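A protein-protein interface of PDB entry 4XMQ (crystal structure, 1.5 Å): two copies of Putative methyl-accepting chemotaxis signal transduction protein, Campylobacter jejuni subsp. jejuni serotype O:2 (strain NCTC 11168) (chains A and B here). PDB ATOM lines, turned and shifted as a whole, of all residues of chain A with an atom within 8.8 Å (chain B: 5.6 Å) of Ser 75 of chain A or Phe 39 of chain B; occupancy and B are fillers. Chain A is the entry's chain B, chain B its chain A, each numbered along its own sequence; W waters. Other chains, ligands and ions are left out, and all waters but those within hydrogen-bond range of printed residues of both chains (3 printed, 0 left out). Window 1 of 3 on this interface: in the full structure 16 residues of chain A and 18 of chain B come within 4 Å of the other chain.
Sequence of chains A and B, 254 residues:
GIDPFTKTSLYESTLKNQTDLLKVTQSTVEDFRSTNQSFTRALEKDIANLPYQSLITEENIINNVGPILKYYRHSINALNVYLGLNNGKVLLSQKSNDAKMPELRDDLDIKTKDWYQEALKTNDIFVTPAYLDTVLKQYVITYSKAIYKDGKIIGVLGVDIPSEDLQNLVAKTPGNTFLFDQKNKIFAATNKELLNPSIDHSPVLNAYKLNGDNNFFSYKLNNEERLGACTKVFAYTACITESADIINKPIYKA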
ATOM      1  N   PHE A  39      38.874 -20.208 -17.481  1.00  0.00           N
ATOM      2  CA  PHE A  39      37.824 -21.219 -17.684  1.00  0.00           C
ATOM      3  C   PHE A  39      38.247 -22.143 -18.826  1.00  0.00           C
ATOM      4  O   PHE A  39      38.123 -23.353 -18.733  1.00  0.00           O
ATOM      5  CB  PHE A  39      36.517 -20.489 -18.048  1.00  0.00           C
ATOM      6  CG  PHE A  39      35.414 -21.390 -18.524  1.00  0.00           C
ATOM      7  CD1 PHE A  39      34.543 -22.029 -17.631  1.00  0.00           C
ATOM      8  CD2 PHE A  39      35.193 -21.571 -19.886  1.00  0.00           C
ATOM      9  CE1 PHE A  39      33.513 -22.800 -18.108  1.00  0.00           C
ATOM     10  CE2 PHE A  39      34.151 -22.337 -20.366  1.00  0.00           C
ATOM     11  CZ  PHE A  39      33.319 -22.960 -19.470  1.00  0.00           C
ATOM     12  N   ALA A  42      41.091 -24.476 -17.910  1.00  0.00           N
ATOM     13  CA  ALA A  42      40.593 -25.566 -17.037  1.00  0.00           C
ATOM     14  C   ALA A  42      39.914 -26.649 -17.884  1.00  0.00           C
ATOM     15  O   ALA A  42      40.117 -27.826 -17.698  1.00  0.00           O
ATOM     16  CB  ALA A  42      39.673 -25.015 -15.941  1.00  0.00           C
ATOM     17  N   LEU A  43      39.086 -26.209 -18.852  1.00  0.00           N
ATOM     18  CA  LEU A  43      38.417 -27.137 -19.723  1.00  0.00           C
ATOM     19  C   LEU A  43      39.404 -27.985 -20.536  1.00  0.00           C
ATOM     20  O   LEU A  43      39.276 -29.212 -20.603  1.00  0.00           O
ATOM     21  CB  LEU A  43      37.474 -26.392 -20.636  1.00  0.00           C
ATOM     22  CG  LEU A  43      36.612 -27.193 -21.612  1.00  0.00           C
ATOM     23  CD1 LEU A  43      35.975 -28.371 -20.918  1.00  0.00           C
ATOM     24  CD2 LEU A  43      35.547 -26.256 -22.159  1.00  0.00           C
ATOM     25  N   ILE A  68      31.727 -33.373 -20.694  1.00  0.00           N
ATOM     26  CA  ILE A  68      32.587 -32.349 -20.127  1.00  0.00           C
ATOM     27  C   ILE A  68      32.310 -30.965 -20.732  1.00  0.00           C
ATOM     28  O   ILE A  68      32.191 -29.988 -20.002  1.00  0.00           O
ATOM     29  CB  ILE A  68      34.091 -32.676 -20.321  1.00  0.00           C
ATOM     30  CG1 ILE A  68      34.330 -34.111 -19.856  1.00  0.00           C
ATOM     31  CG2 ILE A  68      34.913 -31.654 -19.588  1.00  0.00           C
ATOM     32  CD1 ILE A  68      35.787 -34.593 -19.958  1.00  0.00           C
ATOM     33  N   LEU A  69      32.090 -30.914 -22.046  1.00  0.00           N
ATOM     34  CA  LEU A  69      31.743 -29.655 -22.720  1.00  0.00           C
ATOM     35  C   LEU A  69      30.417 -29.086 -22.132  1.00  0.00           C
ATOM     36  O   LEU A  69      30.314 -27.887 -21.874  1.00  0.00           O
ATOM     37  CB  LEU A  69      31.606 -29.847 -24.215  1.00  0.00           C
ATOM     38  CG  LEU A  69      32.777 -30.436 -25.001  1.00  0.00           C
ATOM     39  CD1 LEU A  69      32.498 -30.393 -26.508  1.00  0.00           C
ATOM     40  CD2 LEU A  69      34.114 -29.705 -24.752  1.00  0.00           C
ATOM     41  N   LYS A  70      29.423 -29.974 -21.943  1.00  0.00           N
ATOM     42  CA  LYS A  70      28.146 -29.564 -21.481  1.00  0.00           C
ATOM     43  C   LYS A  70      28.165 -29.092 -20.021  1.00  0.00           C
ATOM     44  O   LYS A  70      27.628 -28.046 -19.680  1.00  0.00           O
ATOM     45  CB  LYS A  70      27.147 -30.707 -21.640  1.00  0.00           C
ATOM     46  CG  LYS A  70      25.698 -30.320 -21.363  1.00  0.00           C
ATOM     47  CD  LYS A  70      24.766 -31.440 -21.795  1.00  0.00           C
ATOM     48  CE  LYS A  70      23.340 -30.922 -21.947  1.00  0.00           C
ATOM     49  NZ  LYS A  70      22.411 -32.035 -22.293  1.00  0.00           N
ATOM     50  N   TYR A  71      28.832 -29.866 -19.132  1.00  0.00           N
ATOM     51  CA  TYR A  71      28.964 -29.426 -17.743  1.00  0.00           C
ATOM     52  C   TYR A  71      29.659 -28.053 -17.661  1.00  0.00           C
ATOM     53  O   TYR A  71      29.252 -27.164 -16.936  1.00  0.00           O
ATOM     54  CB  TYR A  71      29.740 -30.494 -16.925  1.00  0.00           C
ATOM     55  CG  TYR A  71      28.964 -31.775 -16.697  1.00  0.00           C
ATOM     56  CD1 TYR A  71      27.634 -31.744 -16.391  1.00  0.00           C
ATOM     57  CD2 TYR A  71      29.567 -33.016 -16.862  1.00  0.00           C
ATOM     58  CE1 TYR A  71      26.898 -32.932 -16.191  1.00  0.00           C
ATOM     59  CE2 TYR A  71      28.869 -34.197 -16.648  1.00  0.00           C
ATOM     60  CZ  TYR A  71      27.550 -34.146 -16.319  1.00  0.00           C
ATOM     61  OH  TYR A  71      26.865 -35.336 -16.066  1.00  0.00           O
ATOM     62  N   TYR A  72      30.756 -27.904 -18.399  1.00  0.00           N
ATOM     63  CA  TYR A  72      31.468 -26.652 -18.424  1.00  0.00           C
ATOM     64  C   TYR A  72      30.613 -25.494 -18.970  1.00  0.00           C
ATOM     65  O   TYR A  72      30.595 -24.401 -18.416  1.00  0.00           O
ATOM     66  CB  TYR A  72      32.772 -26.770 -19.190  1.00  0.00           C
ATOM     67  CG  TYR A  72      33.995 -27.081 -18.270  1.00  0.00           C
ATOM     68  CD1 TYR A  72      34.248 -28.370 -17.821  1.00  0.00           C
ATOM     69  CD2 TYR A  72      34.936 -26.089 -17.997  1.00  0.00           C
ATOM     70  CE1 TYR A  72      35.356 -28.647 -17.037  1.00  0.00           C
ATOM     71  CE2 TYR A  72      36.057 -26.371 -17.211  1.00  0.00           C
ATOM     72  CZ  TYR A  72      36.242 -27.643 -16.735  1.00  0.00           C
ATOM     73  OH  TYR A  72      37.404 -27.886 -16.000  1.00  0.00           O
ATOM     74  N   ARG A  73      29.894 -25.777 -20.064  1.00  0.00           N
ATOM     75  CA  ARG A  73      29.019 -24.763 -20.645  1.00  0.00           C
ATOM     76  C   ARG A  73      28.023 -24.269 -19.574  1.00  0.00           C
ATOM     77  O   ARG A  73      27.800 -23.092 -19.410  1.00  0.00           O
ATOM     78  CB  ARG A  73      28.250 -25.271 -21.843  1.00  0.00           C
ATOM     79  CG  ARG A  73      27.282 -24.242 -22.381  1.00  0.00           C
ATOM     80  CD  ARG A  73      26.656 -24.633 -23.702  1.00  0.00           C
ATOM     81  NE  ARG A  73      25.889 -25.893 -23.705  1.00  0.00           N
ATOM     82  CZ  ARG A  73      24.678 -26.060 -23.216  1.00  0.00           C
ATOM     83  NH1 ARG A  73      24.043 -25.079 -22.574  1.00  0.00           N
ATOM     84  NH2 ARG A  73      24.133 -27.262 -23.246  1.00  0.00           N
ATOM     85  N   HIS A  74      27.410 -25.208 -18.853  1.00  0.00           N
ATOM     86  CA  HIS A  74      26.450 -24.824 -17.817  1.00  0.00           C
ATOM     87  C   HIS A  74      27.077 -24.000 -16.699  1.00  0.00           C
ATOM     88  O   HIS A  74      26.486 -23.060 -16.193  1.00  0.00           O
ATOM     89  CB  HIS A  74      25.811 -26.073 -17.203  1.00  0.00           C
ATOM     90  CG  HIS A  74      24.871 -26.804 -18.102  1.00  0.00           C
ATOM     91  ND1 HIS A  74      24.463 -28.098 -17.872  1.00  0.00           N
ATOM     92  CD2 HIS A  74      24.164 -26.398 -19.179  1.00  0.00           C
ATOM     93  CE1 HIS A  74      23.627 -28.473 -18.813  1.00  0.00           C
ATOM     94  NE2 HIS A  74      23.379 -27.447 -19.578  1.00  0.00           N
ATOM     95  N   SER A  75      28.286 -24.386 -16.296  1.00  0.00           N
ATOM     96  CA  SER A  75      28.878 -23.793 -15.131  1.00  0.00           C
ATOM     97  C   SER A  75      29.024 -22.268 -15.240  1.00  0.00           C
ATOM     98  O   SER A  75      28.904 -21.588 -14.248  1.00  0.00           O
ATOM     99  CB  SER A  75      30.263 -24.438 -14.844  1.00  0.00           C
ATOM    100  OG  SER A  75      31.224 -24.073 -15.798  1.00  0.00           O
ATOM    101  N   ILE A  76      29.288 -21.770 -16.472  1.00  0.00           N
ATOM    102  CA  ILE A  76      29.540 -20.343 -16.697  1.00  0.00           C
ATOM    103  C   ILE A  76      28.429 -19.728 -17.570  1.00  0.00           C
ATOM    104  O   ILE A  76      28.472 -18.513 -17.812  1.00  0.00           O
ATOM    105  CB  ILE A  76      30.918 -20.139 -17.370  1.00  0.00           C
ATOM    106  CG1 ILE A  76      31.505 -18.736 -17.074  1.00  0.00           C
ATOM    107  CG2 ILE A  76      30.907 -20.477 -18.853  1.00  0.00           C
ATOM    108  CD1 ILE A  76      32.942 -18.523 -17.534  1.00  0.00           C
ATOM    109  N   ASN A  77      27.497 -20.538 -18.014  1.00  0.00           N
ATOM    110  CA  ASN A  77      26.439 -20.114 -18.949  1.00  0.00           C
ATOM    111  C   ASN A  77      27.059 -19.605 -20.238  1.00  0.00           C
ATOM    112  O   ASN A  77      26.679 -18.531 -20.750  1.00  0.00           O
ATOM    113  CB  ASN A  77      25.563 -19.102 -18.289  1.00  0.00           C
ATOM    114  CG  ASN A  77      24.240 -18.875 -19.058  1.00  0.00           C
ATOM    115  OD1 ASN A  77      23.791 -19.717 -19.812  1.00  0.00           O
ATOM    116  ND2 ASN A  77      23.673 -17.703 -18.883  1.00  0.00           N
ATOM    117  N   ALA A  78      27.976 -20.380 -20.807  1.00  0.00           N
ATOM    118  CA  ALA A  78      28.547 -20.051 -22.106  1.00  0.00           C
ATOM    119  C   ALA A  78      27.457 -20.200 -23.189  1.00  0.00           C
ATOM    120  O   ALA A  78      26.510 -20.967 -23.032  1.00  0.00           O
ATOM    121  CB  ALA A  78      29.722 -20.965 -22.409  1.00  0.00           C
ATOM    122  N   VAL A  81      30.127 -24.293 -26.425  1.00  0.00           N
ATOM    123  CA  VAL A  81      31.413 -24.920 -26.082  1.00  0.00           C
ATOM    124  C   VAL A  81      31.604 -26.074 -27.039  1.00  0.00           C
ATOM    125  O   VAL A  81      30.674 -26.887 -27.210  1.00  0.00           O
ATOM    126  CB  VAL A  81      31.452 -25.383 -24.621  1.00  0.00           C
ATOM    127  CG1 VAL A  81      32.728 -26.119 -24.319  1.00  0.00           C
ATOM    128  CG2 VAL A  81      31.241 -24.230 -23.678  1.00  0.00           C
ATOM    129  N   ASP A  98      19.536 -27.283 -25.173  1.00  0.00           N
ATOM    130  CA  ASP A  98      20.188 -27.881 -24.014  1.00  0.00           C
ATOM    131  C   ASP A  98      19.752 -29.332 -23.682  1.00  0.00           C
ATOM    132  O   ASP A  98      20.441 -30.035 -22.941  1.00  0.00           O
ATOM    133  CB  ASP A  98      19.932 -26.976 -22.815  1.00  0.00           C
ATOM    134  CG  ASP A  98      20.648 -27.447 -21.593  1.00  0.00           C
ATOM    135  OD1 ASP A  98      21.871 -27.264 -21.551  1.00  0.00           O
ATOM    136  OD2 ASP A  98      20.020 -28.027 -20.711  1.00  0.00           O
ATOM    137  N   ILE A 161      31.539 -16.919 -25.230  1.00  0.00           N
ATOM    138  CA  ILE A 161      30.895 -16.275 -24.086  1.00  0.00           C
ATOM    139  C   ILE A 161      29.941 -15.190 -24.547  1.00  0.00           C
ATOM    140  O   ILE A 161      30.316 -14.424 -25.402  1.00  0.00           O
ATOM    141  CB  ILE A 161      31.904 -15.719 -23.103  1.00  0.00           C
ATOM    142  CG1 ILE A 161      32.878 -16.809 -22.642  1.00  0.00           C
ATOM    143  CG2 ILE A 161      31.207 -15.045 -21.896  1.00  0.00           C
ATOM    144  CD1 ILE A 161      32.230 -17.957 -21.922  1.00  0.00           C
ATOM    145  N   SER B  34      26.798 -12.854  -7.142  1.00  0.00           N
ATOM    146  CA  SER B  34      25.876 -13.359  -8.171  1.00  0.00           C
ATOM    147  C   SER B  34      26.538 -14.390  -9.086  1.00  0.00           C
ATOM    148  O   SER B  34      25.906 -15.346  -9.534  1.00  0.00           O
ATOM    149  CB  SER B  34      25.243 -12.209  -8.946  1.00  0.00           C
ATOM    150  OG  SER B  34      26.194 -11.490  -9.681  1.00  0.00           O
ATOM    151  N   THR B  35      27.826 -14.213  -9.346  1.00  0.00           N
ATOM    152  CA  THR B  35      28.567 -15.175 -10.141  1.00  0.00           C
ATOM    153  C   THR B  35      28.622 -16.540  -9.446  1.00  0.00           C
ATOM    154  O   THR B  35      28.375 -17.575 -10.046  1.00  0.00           O
ATOM    155  CB  THR B  35      29.954 -14.660 -10.483  1.00  0.00           C
ATOM    156  OG1 THR B  35      29.783 -13.577 -11.425  1.00  0.00           O
ATOM    157  CG2 THR B  35      30.788 -15.735 -11.105  1.00  0.00           C
ATOM    158  N   ASN B  36      28.918 -16.510  -8.162  1.00  0.00           N
ATOM    159  CA  ASN B  36      29.000 -17.725  -7.386  1.00  0.00           C
ATOM    160  C   ASN B  36      27.635 -18.377  -7.201  1.00  0.00           C
ATOM    161  O   ASN B  36      27.506 -19.593  -7.196  1.00  0.00           O
ATOM    162  CB  ASN B  36      29.665 -17.416  -6.037  1.00  0.00           C
ATOM    163  CG  ASN B  36      31.108 -17.081  -6.195  1.00  0.00           C
ATOM    164  OD1 ASN B  36      31.730 -17.578  -7.133  1.00  0.00           O
ATOM    165  ND2 ASN B  36      31.667 -16.297  -5.296  1.00  0.00           N
ATOM    166  N   GLN B  37      26.582 -17.568  -7.047  1.00  0.00           N
ATOM    167  CA  GLN B  37      25.200 -18.116  -6.974  1.00  0.00           C
ATOM    168  C   GLN B  37      24.763 -18.754  -8.282  1.00  0.00           C
ATOM    169  O   GLN B  37      24.163 -19.838  -8.288  1.00  0.00           O
ATOM    170  CB  GLN B  37      24.226 -17.015  -6.573  1.00  0.00           C
ATOM    171  CG  GLN B  37      24.325 -16.537  -5.143  1.00  0.00           C
ATOM    172  CD  GLN B  37      23.526 -15.228  -4.909  1.00  0.00           C
ATOM    173  OE1 GLN B  37      23.569 -14.344  -5.751  1.00  0.00           O
ATOM    174  NE2 GLN B  37      22.903 -15.086  -3.773  1.00  0.00           N
ATOM    175  N   SER B  38      25.020 -18.107  -9.414  1.00  0.00           N
ATOM    176  CA  SER B  38      24.718 -18.678 -10.703  1.00  0.00           C
ATOM    177  C   SER B  38      25.382 -20.044 -10.964  1.00  0.00           C
ATOM    178  O   SER B  38      24.760 -20.983 -11.414  1.00  0.00           O
ATOM    179  CB  SER B  38      25.095 -17.711 -11.840  1.00  0.00           C
ATOM    180  OG  SER B  38      24.264 -16.557 -11.832  1.00  0.00           O
ATOM    181  N   PHE B  39      26.649 -20.126 -10.558  1.00  0.00           N
ATOM    182  CA  PHE B  39      27.453 -21.322 -10.629  1.00  0.00           C
ATOM    183  C   PHE B  39      26.762 -22.427  -9.804  1.00  0.00           C
ATOM    184  O   PHE B  39      26.563 -23.525 -10.277  1.00  0.00           O
ATOM    185  CB  PHE B  39      28.840 -21.023 -10.096  1.00  0.00           C
ATOM    186  CG  PHE B  39      29.706 -22.218  -9.901  1.00  0.00           C
ATOM    187  CD1 PHE B  39      30.499 -22.697 -10.905  1.00  0.00           C
ATOM    188  CD2 PHE B  39      29.761 -22.849  -8.649  1.00  0.00           C
ATOM    189  CE1 PHE B  39      31.331 -23.764 -10.711  1.00  0.00           C
ATOM    190  CE2 PHE B  39      30.598 -23.952  -8.473  1.00  0.00           C
ATOM    191  CZ  PHE B  39      31.396 -24.378  -9.480  1.00  0.00           C
ATOM    192  N   THR B  40      26.429 -22.082  -8.573  1.00  0.00           N
ATOM    193  CA  THR B  40      25.840 -23.070  -7.629  1.00  0.00           C
ATOM    194  C   THR B  40      24.522 -23.579  -8.181  1.00  0.00           C
ATOM    195  O   THR B  40      24.225 -24.758  -8.076  1.00  0.00           O
ATOM    196  CB  THR B  40      25.670 -22.414  -6.231  1.00  0.00           C
ATOM    197  OG1 THR B  40      26.945 -21.974  -5.752  1.00  0.00           O
ATOM    198  CG2 THR B  40      25.074 -23.396  -5.215  1.00  0.00           C
ATOM    199  N   ARG B  41      23.702 -22.678  -8.707  1.00  0.00           N
ATOM    200  CA  ARG B  41      22.407 -23.031  -9.267  1.00  0.00           C
ATOM    201  C   ARG B  41      22.542 -23.949 -10.456  1.00  0.00           C
ATOM    202  O   ARG B  41      21.773 -24.905 -10.636  1.00  0.00           O
ATOM    203  CB  ARG B  41      21.601 -21.763  -9.571  1.00  0.00           C
ATOM    204  CG  ARG B  41      20.341 -21.959 -10.318  1.00  0.00           C
ATOM    205  CD  ARG B  41      19.393 -20.794 -10.109  1.00  0.00           C
ATOM    206  NE  ARG B  41      18.900 -20.807  -8.761  1.00  0.00           N
ATOM    207  CZ  ARG B  41      19.194 -19.925  -7.791  1.00  0.00           C
ATOM    208  NH1 ARG B  41      19.920 -18.831  -8.045  1.00  0.00           N
ATOM    209  NH2 ARG B  41      18.638 -20.148  -6.590  1.00  0.00           N
ATOM    210  N   ALA B  42      23.502 -23.649 -11.339  1.00  0.00           N
ATOM    211  CA  ALA B  42      23.788 -24.507 -12.455  1.00  0.00           C
ATOM    212  C   ALA B  42      24.162 -25.932 -12.037  1.00  0.00           C
ATOM    213  O   ALA B  42      23.711 -26.911 -12.610  1.00  0.00           O
ATOM    214  CB  ALA B  42      24.845 -23.864 -13.336  1.00  0.00           C
ATOM    215  N   LEU B  43      24.989 -26.002 -11.013  1.00  0.00           N
ATOM    216  CA  LEU B  43      25.444 -27.303 -10.478  1.00  0.00           C
ATOM    217  C   LEU B  43      24.276 -28.062  -9.890  1.00  0.00           C
ATOM    218  O   LEU B  43      24.097 -29.241 -10.160  1.00  0.00           O
ATOM    219  CB  LEU B  43      26.555 -27.078  -9.475  1.00  0.00           C
ATOM    220  CG  LEU B  43      27.168 -28.327  -8.848  1.00  0.00           C
ATOM    221  CD1 LEU B  43      27.463 -29.385  -9.868  1.00  0.00           C
ATOM    222  CD2 LEU B  43      28.429 -27.908  -8.118  1.00  0.00           C
ATOM    223  N   GLU B  44      23.419 -27.342  -9.163  1.00  0.00           N
ATOM    224  CA  GLU B  44      22.193 -27.935  -8.621  1.00  0.00           C
ATOM    225  C   GLU B  44      21.375 -28.545  -9.743  1.00  0.00           C
ATOM    226  O   GLU B  44      20.818 -29.664  -9.610  1.00  0.00           O
ATOM    227  CB  GLU B  44      21.370 -26.872  -7.899  1.00  0.00           C
ATOM    228  CG  GLU B  44      19.922 -27.265  -7.639  1.00  0.00           C
ATOM    229  CD  GLU B  44      19.070 -26.145  -7.079  1.00  0.00           C
ATOM    230  OE1 GLU B  44      19.193 -24.992  -7.570  1.00  0.00           O
ATOM    231  OE2 GLU B  44      18.345 -26.362  -6.096  1.00  0.00           O
ATOM    232  N   ASP B  46      22.251 -29.501 -12.764  1.00  0.00           N
ATOM    233  CA  ASP B  46      22.908 -30.654 -13.404  1.00  0.00           C
ATOM    234  C   ASP B  46      22.827 -31.922 -12.542  1.00  0.00           C
ATOM    235  O   ASP B  46      22.648 -33.008 -13.080  1.00  0.00           O
ATOM    236  CB  ASP B  46      24.358 -30.344 -13.729  1.00  0.00           C
ATOM    237  CG  ASP B  46      24.559 -29.932 -15.169  1.00  0.00           C
ATOM    238  OD1 ASP B  46      23.882 -30.498 -16.051  1.00  0.00           O
ATOM    239  OD2 ASP B  46      25.463 -29.106 -15.443  1.00  0.00           O
ATOM    240  N   TYR B  72      32.967 -28.851 -12.267  1.00  0.00           N
ATOM    241  CA  TYR B  72      32.522 -27.570 -11.772  1.00  0.00           C
ATOM    242  C   TYR B  72      33.594 -26.904 -10.914  1.00  0.00           C
ATOM    243  O   TYR B  72      33.901 -25.726 -11.082  1.00  0.00           O
ATOM    244  CB  TYR B  72      31.211 -27.671 -11.036  1.00  0.00           C
ATOM    245  CG  TYR B  72      29.973 -27.504 -11.949  1.00  0.00           C
ATOM    246  CD1 TYR B  72      29.558 -28.494 -12.805  1.00  0.00           C
ATOM    247  CD2 TYR B  72      29.178 -26.375 -11.849  1.00  0.00           C
ATOM    248  CE1 TYR B  72      28.422 -28.351 -13.595  1.00  0.00           C
ATOM    249  CE2 TYR B  72      28.088 -26.204 -12.649  1.00  0.00           C
ATOM    250  CZ  TYR B  72      27.676 -27.195 -13.469  1.00  0.00           C
ATOM    251  OH  TYR B  72      26.519 -27.021 -14.223  1.00  0.00           O
ATOM    252  N   ARG B  73      34.194 -27.672 -10.005  1.00  0.00           N
ATOM    253  CA  ARG B  73      35.270 -27.141  -9.193  1.00  0.00           C
ATOM    254  C   ARG B  73      36.374 -26.545 -10.079  1.00  0.00           C
ATOM    255  O   ARG B  73      36.836 -25.434  -9.856  1.00  0.00           O
ATOM    256  CB  ARG B  73      35.827 -28.219  -8.259  1.00  0.00           C
ATOM    257  CG  ARG B  73      37.054 -27.730  -7.515  1.00  0.00           C
ATOM    258  CD  ARG B  73      37.556 -28.689  -6.419  1.00  0.00           C
ATOM    259  NE  ARG B  73      37.977 -29.962  -6.911  1.00  0.00           N
ATOM    260  CZ  ARG B  73      39.131 -30.238  -7.496  1.00  0.00           C
ATOM    261  NH1 ARG B  73      40.015 -29.264  -7.726  1.00  0.00           N
ATOM    262  NH2 ARG B  73      39.400 -31.481  -7.886  1.00  0.00           N
ATOM    263  N   SER B  75      36.215 -25.553 -13.158  1.00  0.00           N
ATOM    264  CA  SER B  75      35.799 -24.474 -14.019  1.00  0.00           C
ATOM    265  C   SER B  75      35.940 -23.093 -13.380  1.00  0.00           C
ATOM    266  O   SER B  75      36.215 -22.102 -14.099  1.00  0.00           O
ATOM    267  CB  SER B  75      34.339 -24.709 -14.470  1.00  0.00           C
ATOM    268  OG  SER B  75      33.420 -24.464 -13.431  1.00  0.00           O
ATOM    269  N   ILE B  76      35.761 -23.009 -12.055  1.00  0.00           N
ATOM    270  CA  ILE B  76      35.790 -21.767 -11.309  1.00  0.00           C
ATOM    271  C   ILE B  76      36.980 -21.698 -10.331  1.00  0.00           C
ATOM    272  O   ILE B  76      37.150 -20.691  -9.614  1.00  0.00           O
ATOM    273  CB  ILE B  76      34.431 -21.534 -10.585  1.00  0.00           C
ATOM    274  CG1 ILE B  76      34.167 -20.042 -10.296  1.00  0.00           C
ATOM    275  CG2 ILE B  76      34.333 -22.388  -9.318  1.00  0.00           C
ATOM    276  CD1 ILE B  76      32.718 -19.713  -9.925  1.00  0.00           C
ATOM    277  N   ALA B  78      37.386 -23.463  -7.548  1.00  0.00           N
ATOM    278  CA  ALA B  78      36.882 -23.462  -6.175  1.00  0.00           C
ATOM    279  C   ALA B  78      37.811 -24.290  -5.281  1.00  0.00           C
ATOM    280  O   ALA B  78      38.546 -25.119  -5.763  1.00  0.00           O
ATOM    281  CB  ALA B  78      35.450 -23.958  -6.116  1.00  0.00           C
ATOM    282  N   VAL B  81      34.103 -28.544  -3.633  1.00  0.00           N
ATOM    283  CA  VAL B  81      32.748 -28.663  -4.100  1.00  0.00           C
ATOM    284  C   VAL B  81      32.264 -30.024  -3.556  1.00  0.00           C
ATOM    285  O   VAL B  81      32.935 -31.016  -3.733  1.00  0.00           O
ATOM    286  CB  VAL B  81      32.657 -28.563  -5.627  1.00  0.00           C
ATOM    287  CG1 VAL B  81      31.220 -28.748  -6.116  1.00  0.00           C
ATOM    288  CG2 VAL B  81      33.191 -27.199  -6.112  1.00  0.00           C
ATOM    289  N   VAL B 159      29.712 -25.212  -1.934  1.00  0.00           N
ATOM    290  CA  VAL B 159      30.790 -24.671  -2.756  1.00  0.00           C
ATOM    291  C   VAL B 159      31.601 -23.688  -1.910  1.00  0.00           C
ATOM    292  O   VAL B 159      31.060 -22.724  -1.382  1.00  0.00           O
ATOM    293  CB  VAL B 159      30.225 -23.942  -3.984  1.00  0.00           C
ATOM    294  CG1 VAL B 159      31.346 -23.275  -4.802  1.00  0.00           C
ATOM    295  CG2 VAL B 159      29.352 -24.818  -4.853  1.00  0.00           C
HETATM  296  O   HOH W   1      32.369 -21.881 -14.353  1.00  0.00           O
HETATM  297  O   HOH W   2      23.023 -26.623 -15.299  1.00  0.00           O
HETATM  298  O   HOH W   3      21.434 -28.723 -16.275  1.00  0.00           O
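OD2 of Asp 46 of chain B is in hydrogen-bond range of ND1 of His 74 of chain A (2.8 Å). The side-chain hydroxyl (OG) of Ser 75 of chain A is in hydrogen-bond range of the side-chain hydroxyl (OG) of Ser 75 of chain B, at 3.3 Å.
Leu 43 of chain A touches none of the printed residues of chain B. Of the printed residues of chain B, Tyr 71 of chain A touches Asp 46 and Tyr 72. Of the printed residues of chain B, Tyr 72 of chain A touches Ser 75. Ser 75 of chain A touches just these residues of chain B: Phe 39 (3.9 Å), Tyr 72 (3.5 Å) and Ser 75 (3.3 Å). No residue of chain A comes within 4 Å of Ser 38 of chain B. Phe 39 of chain B touches one residue of chain A. Of the printed residues of chain A, Ala 42 of chain B touches His 74. Of the printed residues of chain A, Asp 46 of chain B touches Tyr 71 and His 74. Printed residues of chain A within 4 Å of Tyr 72 of chain B: Tyr 71, His 74 and Ser 75. Val 159 of chain B touches none of the printed residues of chain A. The nearest residue of chain A that does not touch Phe 39 of chain B is Ile 76 of chain A (5.8 Å).
Of the 17 printed residues of chain A, 5 touch a printed residue of chain B. Hydrophobic or aromatic side chains of chain B within 4 Å of the printed part of chain A: Phe 39, Ala 42 and Tyr 72. Among the printed residues, 10 pairs touch across the chains.
Water W2 lies within hydrogen-bond range of O of Ala 42 of chain B (2.8 Å), ND1 of His 74 of chain A (3.3 Å) and OD2 of Asp 46 of chain B (3.5 Å). Water W1 lies within hydrogen-bond range of OG of Ser 75 of chain A (2.9 Å) and OG of Ser 75 of chain B (2.9 Å). Water W3 bridges the side-chain carboxylate (OD1) of Asp 46 of chain B (3.0 Å) and a ring nitrogen (ND1) of His 74 of chain A (3.5 Å).
The side-chain hydroxyl (OH) of Tyr 72 of chain B is in hydrogen-bond range of the backbone carbonyl oxygen (O) of Ala 42 of chain B (3.2 Å). The side-chain carboxylate (OD2) of Asp 46 of chain B lies within hydrogen-bond range of the side-chain hydroxyl (OH) of Tyr 72 of chain B (2.6 Å). O of Ala 42 of chain A lies within hydrogen-bond range of OH of Tyr 72 of chain A (3.2 Å). The backbone carbonyl oxygen of Tyr 72 of chain A is in hydrogen-bond range of the side-chain hydroxyl of Ser 75 of chain A (2.7 Å). NE2 of His 74 of chain A is in hydrogen-bond range of OD1 of Asp 98 of chain A (2.5 Å).
Phe 39 of chain A touches Ser 75 of chain B, and with the chains exchanged Ser 75 of chain A touches Phe 39 of chain B. Tyr 72 of chain A touches Ser 75 of chain B, and with the chains exchanged Ser 75 of chain A touches Tyr 72 of chain B. Ser 75 of chain B touches its own counterpart, Ser 75 of chain A. 9 positions are printed for both chains.
Ser 75 of chain B touches Phe 39 of chain A. Tyr 71 of chain A touches Asp 46 of chain B (CD1 to OD2, 3.5 Å). CE1 of Tyr 72 of chain B touches O of Tyr 71 of chain A, at 3.6 Å. CE2 of Tyr 72 of chain A touches CB of Ser 75 of chain B (3.6 Å). O of His 74 of chain A touches CB of Ala 42 of chain B (3.4 Å). OH of Tyr 72 of chain B touches CB of His 74 of chain A, 3.2 Å away. Phe 39 of chain B touches Ser 75 of chain A. Tyr 72 of chain B touches Ser 75 of chain A (CE2 to CA, 3.5 Å).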
